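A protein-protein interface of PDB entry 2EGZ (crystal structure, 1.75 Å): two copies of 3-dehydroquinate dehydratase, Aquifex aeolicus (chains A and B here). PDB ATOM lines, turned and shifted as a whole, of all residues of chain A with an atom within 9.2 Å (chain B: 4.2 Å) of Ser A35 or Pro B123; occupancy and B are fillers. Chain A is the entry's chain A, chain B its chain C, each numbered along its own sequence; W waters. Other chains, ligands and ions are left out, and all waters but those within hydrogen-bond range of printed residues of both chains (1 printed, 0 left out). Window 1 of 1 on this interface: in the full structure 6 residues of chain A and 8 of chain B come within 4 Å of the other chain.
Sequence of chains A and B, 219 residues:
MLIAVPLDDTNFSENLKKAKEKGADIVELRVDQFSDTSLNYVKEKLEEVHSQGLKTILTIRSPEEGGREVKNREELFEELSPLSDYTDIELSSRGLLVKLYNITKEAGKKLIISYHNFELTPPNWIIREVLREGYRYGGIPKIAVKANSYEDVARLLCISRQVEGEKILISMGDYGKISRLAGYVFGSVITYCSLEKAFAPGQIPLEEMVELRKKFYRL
OH of Tyr B115 is in hydrogen-bond range of OG of Ser A35 (3.5 Å).
The guanidinium group (NE) of Arg A68 lies within hydrogen-bond range of the backbone carbonyl oxygen (O) of Asp A32 (2.9 Å).
O of Phe A34 is in hydrogen-bond range of NH1 of Arg A68, 2.8 Å away.
The backbone NH (N) of Ser A35 lies within hydrogen-bond range of the side-chain carboxylate (OD2) of Asp A9.
ND2 of Asn B117 is in hydrogen-bond range of OH of Tyr B115 (3.2 Å).
Among the printed residues, merely in contact across the chains: Ser A35 with Asn B117, Ser A35 with Pro B123, Ser A35 with Ile B126 and Arg A68 with Trp B125.
Asp A8 touches none of the printed residues of chain B.
Ser A35 touches four residues of chain B.
Of the printed residues of chain A, Tyr B115 touches Ser A35.
Of the printed residues of chain A, Asn B117 touches Ser A35.
Of the printed residues of chain A, Pro B123 touches Ser A35.
Asn B124 touches none of the printed residues of chain A.
Printed residues of chain A within 4 Å of Trp B125: Arg A68.
The nearest residue of chain B that does not touch Ser A35 is Pro B122 (4.1 Å).
Printed residues of chain B that touch a printed residue of chain A: Tyr B115, Asn B117, Pro B123, Trp B125 and Ile B126.
Hydrophobic or aromatic side chains of chain B within 4 Å of the printed part of chain A: Tyr B115, Pro B123, Trp B125 and Ile B126.
Printed residues of chain A that touch a printed residue of chain B: Ser A35 and Arg A68.
Among the printed residues, 5 pairs touch across the chains.
Among the printed residues, no Asp or Glu carboxylate lies within 4 Å of a Lys or Arg side-chain nitrogen of the other chain.
No position is printed for both chains.
Water W1 lies within hydrogen-bond range of the side-chain carboxylate (OD2) of Asp A9 (2.6 Å), the side-chain amide nitrogen (ND2) of Asn B117 (3.1 Å) and the side-chain hydroxyl (OH) of Tyr A41 (3.3 Å).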
ATOM      1  N   ASP A   8     -28.632   5.694   0.556  1.00  0.00           N
ATOM      2  CA  ASP A   8     -27.609   4.689   0.786  1.00  0.00           C
ATOM      3  C   ASP A   8     -27.638   3.896  -0.513  1.00  0.00           C
ATOM      4  O   ASP A   8     -28.199   4.365  -1.500  1.00  0.00           O
ATOM      5  CB  ASP A   8     -27.927   3.786   1.991  1.00  0.00           C
ATOM      6  CG  ASP A   8     -29.298   3.142   1.912  1.00  0.00           C
ATOM      7  OD1 ASP A   8     -29.758   2.819   0.796  1.00  0.00           O
ATOM      8  OD2 ASP A   8     -29.912   2.941   2.984  1.00  0.00           O
ATOM      9  N   ASP A   9     -27.060   2.702  -0.529  1.00  0.00           N
ATOM     10  CA  ASP A   9     -27.041   1.919  -1.760  1.00  0.00           C
ATOM     11  C   ASP A   9     -28.244   0.998  -1.980  1.00  0.00           C
ATOM     12  O   ASP A   9     -28.311   0.293  -2.984  1.00  0.00           O
ATOM     13  CB  ASP A   9     -25.738   1.115  -1.829  1.00  0.00           C
ATOM     14  CG  ASP A   9     -25.540   0.215  -0.625  1.00  0.00           C
ATOM     15  OD1 ASP A   9     -26.186   0.458   0.419  1.00  0.00           O
ATOM     16  OD2 ASP A   9     -24.727  -0.727  -0.716  1.00  0.00           O
ATOM     17  N   THR A  10     -29.202   1.022  -1.061  1.00  0.00           N
ATOM     18  CA  THR A  10     -30.387   0.175  -1.177  1.00  0.00           C
ATOM     19  C   THR A  10     -31.366   0.654  -2.256  1.00  0.00           C
ATOM     20  O   THR A  10     -31.833   1.793  -2.218  1.00  0.00           O
ATOM     21  CB  THR A  10     -31.135   0.105   0.168  1.00  0.00           C
ATOM     22  OG1 THR A  10     -30.235  -0.338   1.192  1.00  0.00           O
ATOM     23  CG2 THR A  10     -32.299  -0.863   0.078  1.00  0.00           C
ATOM     24  N   ARG A  30     -24.576   8.751   0.746  1.00  0.00           N
ATOM     25  CA  ARG A  30     -24.081   8.472   2.093  1.00  0.00           C
ATOM     26  C   ARG A  30     -23.276   7.172   2.018  1.00  0.00           C
ATOM     27  O   ARG A  30     -23.723   6.105   2.444  1.00  0.00           O
ATOM     28  CB  ARG A  30     -25.246   8.339   3.078  1.00  0.00           C
ATOM     29  CG  ARG A  30     -25.820   9.683   3.531  1.00  0.00           C
ATOM     30  CD  ARG A  30     -24.755  10.524   4.250  1.00  0.00           C
ATOM     31  NE  ARG A  30     -24.312   9.931   5.509  1.00  0.00           N
ATOM     32  CZ  ARG A  30     -24.959  10.054   6.667  1.00  0.00           C
ATOM     33  NH1 ARG A  30     -26.087  10.755   6.735  1.00  0.00           N
ATOM     34  NH2 ARG A  30     -24.481   9.473   7.759  1.00  0.00           N
ATOM     35  N   VAL A  31     -22.079   7.284   1.457  1.00  0.00           N
ATOM     36  CA  VAL A  31     -21.186   6.149   1.274  1.00  0.00           C
ATOM     37  C   VAL A  31     -20.913   5.381   2.566  1.00  0.00           C
ATOM     38  O   VAL A  31     -20.715   4.162   2.544  1.00  0.00           O
ATOM     39  CB  VAL A  31     -19.864   6.624   0.643  1.00  0.00           C
ATOM     40  CG1 VAL A  31     -18.906   5.467   0.494  1.00  0.00           C
ATOM     41  CG2 VAL A  31     -20.151   7.248  -0.730  1.00  0.00           C
ATOM     42  N   ASP A  32     -20.908   6.085   3.692  1.00  0.00           N
ATOM     43  CA  ASP A  32     -20.670   5.431   4.971  1.00  0.00           C
ATOM     44  C   ASP A  32     -21.801   4.449   5.262  1.00  0.00           C
ATOM     45  O   ASP A  32     -21.654   3.548   6.084  1.00  0.00           O
ATOM     46  CB  ASP A  32     -20.582   6.465   6.095  1.00  0.00           C
ATOM     47  CG  ASP A  32     -21.788   7.381   6.139  1.00  0.00           C
ATOM     48  OD1 ASP A  32     -21.896   8.269   5.263  1.00  0.00           O
ATOM     49  OD2 ASP A  32     -22.632   7.209   7.042  1.00  0.00           O
ATOM     50  N   GLN A  33     -22.928   4.631   4.582  1.00  0.00           N
ATOM     51  CA  GLN A  33     -24.086   3.760   4.759  1.00  0.00           C
ATOM     52  C   GLN A  33     -24.144   2.659   3.696  1.00  0.00           C
ATOM     53  O   GLN A  33     -25.077   1.854   3.684  1.00  0.00           O
ATOM     54  CB  GLN A  33     -25.383   4.572   4.706  1.00  0.00           C
ATOM     55  CG  GLN A  33     -25.568   5.562   5.851  1.00  0.00           C
ATOM     56  CD  GLN A  33     -25.520   4.896   7.214  1.00  0.00           C
ATOM     57  OE1 GLN A  33     -24.545   5.041   7.957  1.00  0.00           O
ATOM     58  NE2 GLN A  33     -26.571   4.153   7.547  1.00  0.00           N
ATOM     59  N   PHE A  34     -23.156   2.638   2.807  1.00  0.00           N
ATOM     60  CA  PHE A  34     -23.077   1.638   1.743  1.00  0.00           C
ATOM     61  C   PHE A  34     -22.507   0.323   2.278  1.00  0.00           C
ATOM     62  O   PHE A  34     -21.797   0.307   3.283  1.00  0.00           O
ATOM     63  CB  PHE A  34     -22.158   2.130   0.621  1.00  0.00           C
ATOM     64  CG  PHE A  34     -22.801   3.103  -0.333  1.00  0.00           C
ATOM     65  CD1 PHE A  34     -23.864   3.906   0.064  1.00  0.00           C
ATOM     66  CD2 PHE A  34     -22.306   3.241  -1.624  1.00  0.00           C
ATOM     67  CE1 PHE A  34     -24.421   4.835  -0.815  1.00  0.00           C
ATOM     68  CE2 PHE A  34     -22.854   4.165  -2.506  1.00  0.00           C
ATOM     69  CZ  PHE A  34     -23.915   4.964  -2.096  1.00  0.00           C
ATOM     70  N   SER A  35     -22.812  -0.776   1.597  1.00  0.00           N
ATOM     71  CA  SER A  35     -22.291  -2.078   2.002  1.00  0.00           C
ATOM     72  C   SER A  35     -20.955  -2.290   1.297  1.00  0.00           C
ATOM     73  O   SER A  35     -20.054  -2.950   1.822  1.00  0.00           O
ATOM     74  CB  SER A  35     -23.274  -3.184   1.618  1.00  0.00           C
ATOM     75  OG  SER A  35     -24.462  -3.091   2.383  1.00  0.00           O
ATOM     76  N   ASP A  36     -20.838  -1.720   0.102  1.00  0.00           N
ATOM     77  CA  ASP A  36     -19.622  -1.811  -0.699  1.00  0.00           C
ATOM     78  C   ASP A  36     -19.143  -0.383  -0.946  1.00  0.00           C
ATOM     79  O   ASP A  36     -19.886   0.440  -1.481  1.00  0.00           O
ATOM     80  CB  ASP A  36     -19.921  -2.492  -2.041  1.00  0.00           C
ATOM     81  CG  ASP A  36     -18.667  -2.807  -2.839  1.00  0.00           C
ATOM     82  OD1 ASP A  36     -17.779  -1.935  -2.960  1.00  0.00           O
ATOM     83  OD2 ASP A  36     -18.569  -3.938  -3.367  1.00  0.00           O
ATOM     84  N   THR A  37     -17.910  -0.083  -0.553  1.00  0.00           N
ATOM     85  CA  THR A  37     -17.380   1.259  -0.750  1.00  0.00           C
ATOM     86  C   THR A  37     -16.219   1.279  -1.736  1.00  0.00           C
ATOM     87  O   THR A  37     -15.435   2.227  -1.756  1.00  0.00           O
ATOM     88  CB  THR A  37     -16.922   1.892   0.590  1.00  0.00           C
ATOM     89  OG1 THR A  37     -15.803   1.167   1.115  1.00  0.00           O
ATOM     90  CG2 THR A  37     -18.057   1.868   1.600  1.00  0.00           C
ATOM     91  N   SER A  38     -16.112   0.236  -2.560  1.00  0.00           N
ATOM     92  CA  SER A  38     -15.039   0.178  -3.548  1.00  0.00           C
ATOM     93  C   SER A  38     -15.191   1.325  -4.546  1.00  0.00           C
ATOM     94  O   SER A  38     -16.301   1.773  -4.832  1.00  0.00           O
ATOM     95  CB  SER A  38     -15.052  -1.163  -4.297  1.00  0.00           C
ATOM     96  OG  SER A  38     -16.213  -1.305  -5.100  1.00  0.00           O
ATOM     97  N   TYR A  41     -17.875   0.655  -7.389  1.00  0.00           N
ATOM     98  CA  TYR A  41     -19.265   0.586  -6.962  1.00  0.00           C
ATOM     99  C   TYR A  41     -19.783   1.999  -6.698  1.00  0.00           C
ATOM    100  O   TYR A  41     -20.901   2.341  -7.078  1.00  0.00           O
ATOM    101  CB  TYR A  41     -19.382  -0.256  -5.689  1.00  0.00           C
ATOM    102  CG  TYR A  41     -20.803  -0.522  -5.231  1.00  0.00           C
ATOM    103  CD1 TYR A  41     -21.642  -1.369  -5.952  1.00  0.00           C
ATOM    104  CD2 TYR A  41     -21.301   0.061  -4.065  1.00  0.00           C
ATOM    105  CE1 TYR A  41     -22.939  -1.634  -5.524  1.00  0.00           C
ATOM    106  CE2 TYR A  41     -22.599  -0.200  -3.627  1.00  0.00           C
ATOM    107  CZ  TYR A  41     -23.411  -1.049  -4.361  1.00  0.00           C
ATOM    108  OH  TYR A  41     -24.690  -1.325  -3.932  1.00  0.00           O
ATOM    109  N   VAL A  42     -18.964   2.817  -6.045  1.00  0.00           N
ATOM    110  CA  VAL A  42     -19.367   4.185  -5.734  1.00  0.00           C
ATOM    111  C   VAL A  42     -19.335   5.087  -6.966  1.00  0.00           C
ATOM    112  O   VAL A  42     -20.247   5.889  -7.176  1.00  0.00           O
ATOM    113  CB  VAL A  42     -18.470   4.792  -4.641  1.00  0.00           C
ATOM    114  CG1 VAL A  42     -18.926   6.209  -4.319  1.00  0.00           C
ATOM    115  CG2 VAL A  42     -18.532   3.924  -3.393  1.00  0.00           C
ATOM    116  N   LYS A  45     -22.405   4.732  -8.990  1.00  0.00           N
ATOM    117  CA  LYS A  45     -23.556   5.371  -8.367  1.00  0.00           C
ATOM    118  C   LYS A  45     -23.502   6.877  -8.652  1.00  0.00           C
ATOM    119  O   LYS A  45     -24.517   7.503  -8.957  1.00  0.00           O
ATOM    120  CB  LYS A  45     -23.544   5.125  -6.856  1.00  0.00           C
ATOM    121  CG  LYS A  45     -23.767   3.668  -6.446  1.00  0.00           C
ATOM    122  CD  LYS A  45     -25.193   3.240  -6.724  1.00  0.00           C
ATOM    123  CE  LYS A  45     -25.520   1.866  -6.134  1.00  0.00           C
ATOM    124  NZ  LYS A  45     -24.882   0.740  -6.867  1.00  0.00           N
ATOM    125  N   ARG A  68     -19.463   5.722   9.963  1.00  0.00           N
ATOM    126  CA  ARG A  68     -18.718   4.519  10.310  1.00  0.00           C
ATOM    127  C   ARG A  68     -17.403   4.540   9.562  1.00  0.00           C
ATOM    128  O   ARG A  68     -17.234   5.307   8.615  1.00  0.00           O
ATOM    129  CB  ARG A  68     -19.528   3.258   9.976  1.00  0.00           C
ATOM    130  CG  ARG A  68     -19.895   3.072   8.514  1.00  0.00           C
ATOM    131  CD  ARG A  68     -18.868   2.241   7.761  1.00  0.00           C
ATOM    132  NE  ARG A  68     -19.381   1.817   6.458  1.00  0.00           N
ATOM    133  CZ  ARG A  68     -18.707   1.073   5.586  1.00  0.00           C
ATOM    134  NH1 ARG A  68     -19.266   0.742   4.430  1.00  0.00           N
ATOM    135  NH2 ARG A  68     -17.479   0.660   5.862  1.00  0.00           N
ATOM    136  N   GLU A  69     -16.465   3.706   9.992  1.00  0.00           N
ATOM    137  CA  GLU A  69     -15.163   3.665   9.361  1.00  0.00           C
ATOM    138  C   GLU A  69     -15.206   3.126   7.935  1.00  0.00           C
ATOM    139  O   GLU A  69     -15.833   2.105   7.653  1.00  0.00           O
ATOM    140  CB  GLU A  69     -14.191   2.836  10.211  1.00  0.00           C
ATOM    141  CG  GLU A  69     -12.831   2.617   9.560  1.00  0.00           C
ATOM    142  CD  GLU A  69     -11.802   2.057  10.524  1.00  0.00           C
ATOM    143  OE1 GLU A  69     -12.161   1.174  11.335  1.00  0.00           O
ATOM    144  OE2 GLU A  69     -10.631   2.493  10.463  1.00  0.00           O
ATOM    145  N   VAL A  70     -14.546   3.844   7.036  1.00  0.00           N
ATOM    146  CA  VAL A  70     -14.464   3.454   5.636  1.00  0.00           C
ATOM    147  C   VAL A  70     -12.984   3.413   5.302  1.00  0.00           C
ATOM    148  O   VAL A  70     -12.328   4.447   5.172  1.00  0.00           O
ATOM    149  CB  VAL A  70     -15.199   4.462   4.727  1.00  0.00           C
ATOM    150  CG1 VAL A  70     -15.001   4.090   3.262  1.00  0.00           C
ATOM    151  CG2 VAL A  70     -16.675   4.463   5.067  1.00  0.00           C
ATOM    152  N   LYS A  71     -12.469   2.196   5.177  1.00  0.00           N
ATOM    153  CA  LYS A  71     -11.061   1.961   4.905  1.00  0.00           C
ATOM    154  C   LYS A  71     -10.467   2.703   3.719  1.00  0.00           C
ATOM    155  O   LYS A  71      -9.350   3.216   3.809  1.00  0.00           O
ATOM    156  CB  LYS A  71     -10.815   0.460   4.758  1.00  0.00           C
ATOM    157  CG  LYS A  71     -11.380  -0.363   5.913  1.00  0.00           C
ATOM    158  CD  LYS A  71     -11.041   0.258   7.268  1.00  0.00           C
ATOM    159  CE  LYS A  71     -11.542  -0.600   8.425  1.00  0.00           C
ATOM    160  NZ  LYS A  71     -10.838  -1.915   8.479  1.00  0.00           N
ATOM    161  N   ASN A  72     -11.197   2.764   2.608  1.00  0.00           N
ATOM    162  CA  ASN A  72     -10.682   3.454   1.431  1.00  0.00           C
ATOM    163  C   ASN A  72     -11.287   4.847   1.292  1.00  0.00           C
ATOM    164  O   ASN A  72     -11.499   5.343   0.189  1.00  0.00           O
ATOM    165  CB  ASN A  72     -10.946   2.625   0.167  1.00  0.00           C
ATOM    166  CG  ASN A  72     -12.421   2.502  -0.167  1.00  0.00           C
ATOM    167  OD1 ASN A  72     -13.257   2.280   0.709  1.00  0.00           O
ATOM    168  ND2 ASN A  72     -12.744   2.628  -1.448  1.00  0.00           N
ATOM    169  N   TYR B 115     -32.378  -9.008   7.578  1.00  0.00           N
ATOM    170  CA  TYR B 115     -31.576  -8.091   6.786  1.00  0.00           C
ATOM    171  C   TYR B 115     -31.494  -8.701   5.396  1.00  0.00           C
ATOM    172  O   TYR B 115     -31.144  -9.874   5.257  1.00  0.00           O
ATOM    173  CB  TYR B 115     -30.158  -7.963   7.348  1.00  0.00           C
ATOM    174  CG  TYR B 115     -29.227  -7.246   6.392  1.00  0.00           C
ATOM    175  CD1 TYR B 115     -29.327  -5.871   6.196  1.00  0.00           C
ATOM    176  CD2 TYR B 115     -28.304  -7.956   5.620  1.00  0.00           C
ATOM    177  CE1 TYR B 115     -28.542  -5.218   5.245  1.00  0.00           C
ATOM    178  CE2 TYR B 115     -27.513  -7.313   4.667  1.00  0.00           C
ATOM    179  CZ  TYR B 115     -27.641  -5.945   4.484  1.00  0.00           C
ATOM    180  OH  TYR B 115     -26.889  -5.308   3.517  1.00  0.00           O
ATOM    181  N   ASN B 117     -30.116  -8.192   1.243  1.00  0.00           N
ATOM    182  CA  ASN B 117     -29.309  -7.440   0.289  1.00  0.00           C
ATOM    183  C   ASN B 117     -29.482  -8.178  -1.021  1.00  0.00           C
ATOM    184  O   ASN B 117     -28.936  -9.262  -1.216  1.00  0.00           O
ATOM    185  CB  ASN B 117     -27.827  -7.388   0.673  1.00  0.00           C
ATOM    186  CG  ASN B 117     -27.044  -6.410  -0.202  1.00  0.00           C
ATOM    187  OD1 ASN B 117     -27.168  -6.425  -1.430  1.00  0.00           O
ATOM    188  ND2 ASN B 117     -26.240  -5.558   0.424  1.00  0.00           N
ATOM    189  N   THR B 121     -23.210  -9.928  -1.344  1.00  0.00           N
ATOM    190  CA  THR B 121     -22.969 -10.445  -0.005  1.00  0.00           C
ATOM    191  C   THR B 121     -22.017  -9.427   0.611  1.00  0.00           C
ATOM    192  O   THR B 121     -20.854  -9.325   0.213  1.00  0.00           O
ATOM    193  CB  THR B 121     -22.304 -11.830  -0.054  1.00  0.00           C
ATOM    194  OG1 THR B 121     -23.175 -12.739  -0.740  1.00  0.00           O
ATOM    195  CG2 THR B 121     -22.033 -12.351   1.359  1.00  0.00           C
ATOM    196  N   PRO B 122     -22.500  -8.655   1.593  1.00  0.00           N
ATOM    197  CA  PRO B 122     -21.675  -7.632   2.244  1.00  0.00           C
ATOM    198  C   PRO B 122     -20.442  -8.148   2.972  1.00  0.00           C
ATOM    199  O   PRO B 122     -20.329  -9.344   3.263  1.00  0.00           O
ATOM    200  CB  PRO B 122     -22.668  -6.936   3.174  1.00  0.00           C
ATOM    201  CG  PRO B 122     -23.607  -8.046   3.552  1.00  0.00           C
ATOM    202  CD  PRO B 122     -23.823  -8.762   2.238  1.00  0.00           C
ATOM    203  N   PRO B 123     -19.485  -7.246   3.254  1.00  0.00           N
ATOM    204  CA  PRO B 123     -18.239  -7.574   3.952  1.00  0.00           C
ATOM    205  C   PRO B 123     -18.519  -8.296   5.261  1.00  0.00           C
ATOM    206  O   PRO B 123     -19.597  -8.162   5.836  1.00  0.00           O
ATOM    207  CB  PRO B 123     -17.604  -6.204   4.170  1.00  0.00           C
ATOM    208  CG  PRO B 123     -18.018  -5.468   2.942  1.00  0.00           C
ATOM    209  CD  PRO B 123     -19.480  -5.834   2.827  1.00  0.00           C
ATOM    210  N   ASN B 124     -17.538  -9.050   5.740  1.00  0.00           N
ATOM    211  CA  ASN B 124     -17.711  -9.811   6.967  1.00  0.00           C
ATOM    212  C   ASN B 124     -18.182  -9.024   8.176  1.00  0.00           C
ATOM    213  O   ASN B 124     -19.039  -9.504   8.910  1.00  0.00           O
ATOM    214  CB  ASN B 124     -16.424 -10.560   7.314  1.00  0.00           C
ATOM    215  CG  ASN B 124     -16.004 -11.518   6.220  1.00  0.00           C
ATOM    216  OD1 ASN B 124     -16.821 -11.926   5.391  1.00  0.00           O
ATOM    217  ND2 ASN B 124     -14.732 -11.893   6.216  1.00  0.00           N
ATOM    218  N   TRP B 125     -17.648  -7.820   8.387  1.00  0.00           N
ATOM    219  CA  TRP B 125     -18.049  -7.051   9.560  1.00  0.00           C
ATOM    220  C   TRP B 125     -19.539  -6.732   9.568  1.00  0.00           C
ATOM    221  O   TRP B 125     -20.148  -6.628  10.635  1.00  0.00           O
ATOM    222  CB  TRP B 125     -17.226  -5.758   9.694  1.00  0.00           C
ATOM    223  CG  TRP B 125     -17.518  -4.708   8.674  1.00  0.00           C
ATOM    224  CD1 TRP B 125     -16.907  -4.542   7.466  1.00  0.00           C
ATOM    225  CD2 TRP B 125     -18.496  -3.665   8.779  1.00  0.00           C
ATOM    226  NE1 TRP B 125     -17.439  -3.454   6.814  1.00  0.00           N
ATOM    227  CE2 TRP B 125     -18.414  -2.897   7.596  1.00  0.00           C
ATOM    228  CE3 TRP B 125     -19.428  -3.302   9.760  1.00  0.00           C
ATOM    229  CZ2 TRP B 125     -19.238  -1.786   7.365  1.00  0.00           C
ATOM    230  CZ3 TRP B 125     -20.248  -2.195   9.531  1.00  0.00           C
ATOM    231  CH2 TRP B 125     -20.143  -1.451   8.340  1.00  0.00           C
ATOM    232  N   ILE B 126     -20.124  -6.580   8.383  1.00  0.00           N
ATOM    233  CA  ILE B 126     -21.552  -6.305   8.269  1.00  0.00           C
ATOM    234  C   ILE B 126     -22.333  -7.576   8.599  1.00  0.00           C
ATOM    235  O   ILE B 126     -23.339  -7.529   9.305  1.00  0.00           O
ATOM    236  CB  ILE B 126     -21.911  -5.821   6.846  1.00  0.00           C
ATOM    237  CG1 ILE B 126     -21.348  -4.412   6.636  1.00  0.00           C
ATOM    238  CG2 ILE B 126     -23.423  -5.832   6.647  1.00  0.00           C
ATOM    239  CD1 ILE B 126     -21.656  -3.809   5.277  1.00  0.00           C
ATOM    240  N   ILE B 127     -21.867  -8.714   8.092  1.00  0.00           N
ATOM    241  CA  ILE B 127     -22.529  -9.982   8.382  1.00  0.00           C
ATOM    242  C   ILE B 127     -22.567 -10.191   9.896  1.00  0.00           C
ATOM    243  O   ILE B 127     -23.612 -10.508  10.470  1.00  0.00           O
ATOM    244  CB  ILE B 127     -21.775 -11.167   7.734  1.00  0.00           C
ATOM    245  CG1 ILE B 127     -21.896 -11.077   6.213  1.00  0.00           C
ATOM    246  CG2 ILE B 127     -22.324 -12.498   8.261  1.00  0.00           C
ATOM    247  CD1 ILE B 127     -21.072 -12.092   5.454  1.00  0.00           C
ATOM    248  N   ARG B 155     -18.355 -17.961   2.361  1.00  0.00           N
ATOM    249  CA  ARG B 155     -18.060 -16.870   3.287  1.00  0.00           C
ATOM    250  C   ARG B 155     -19.216 -16.583   4.242  1.00  0.00           C
ATOM    251  O   ARG B 155     -19.019 -16.486   5.454  1.00  0.00           O
ATOM    252  CB  ARG B 155     -17.687 -15.608   2.495  1.00  0.00           C
ATOM    253  CG  ARG B 155     -17.084 -14.485   3.332  1.00  0.00           C
ATOM    254  CD  ARG B 155     -16.327 -13.499   2.442  1.00  0.00           C
ATOM    255  NE  ARG B 155     -17.189 -12.865   1.446  1.00  0.00           N
ATOM    256  CZ  ARG B 155     -18.055 -11.889   1.709  1.00  0.00           C
ATOM    257  NH1 ARG B 155     -18.796 -11.376   0.734  1.00  0.00           N
ATOM    258  NH2 ARG B 155     -18.182 -11.424   2.946  1.00  0.00           N
HETATM  259  O   HOH W   1     -25.646  -3.098  -1.307  1.00  0.00           O
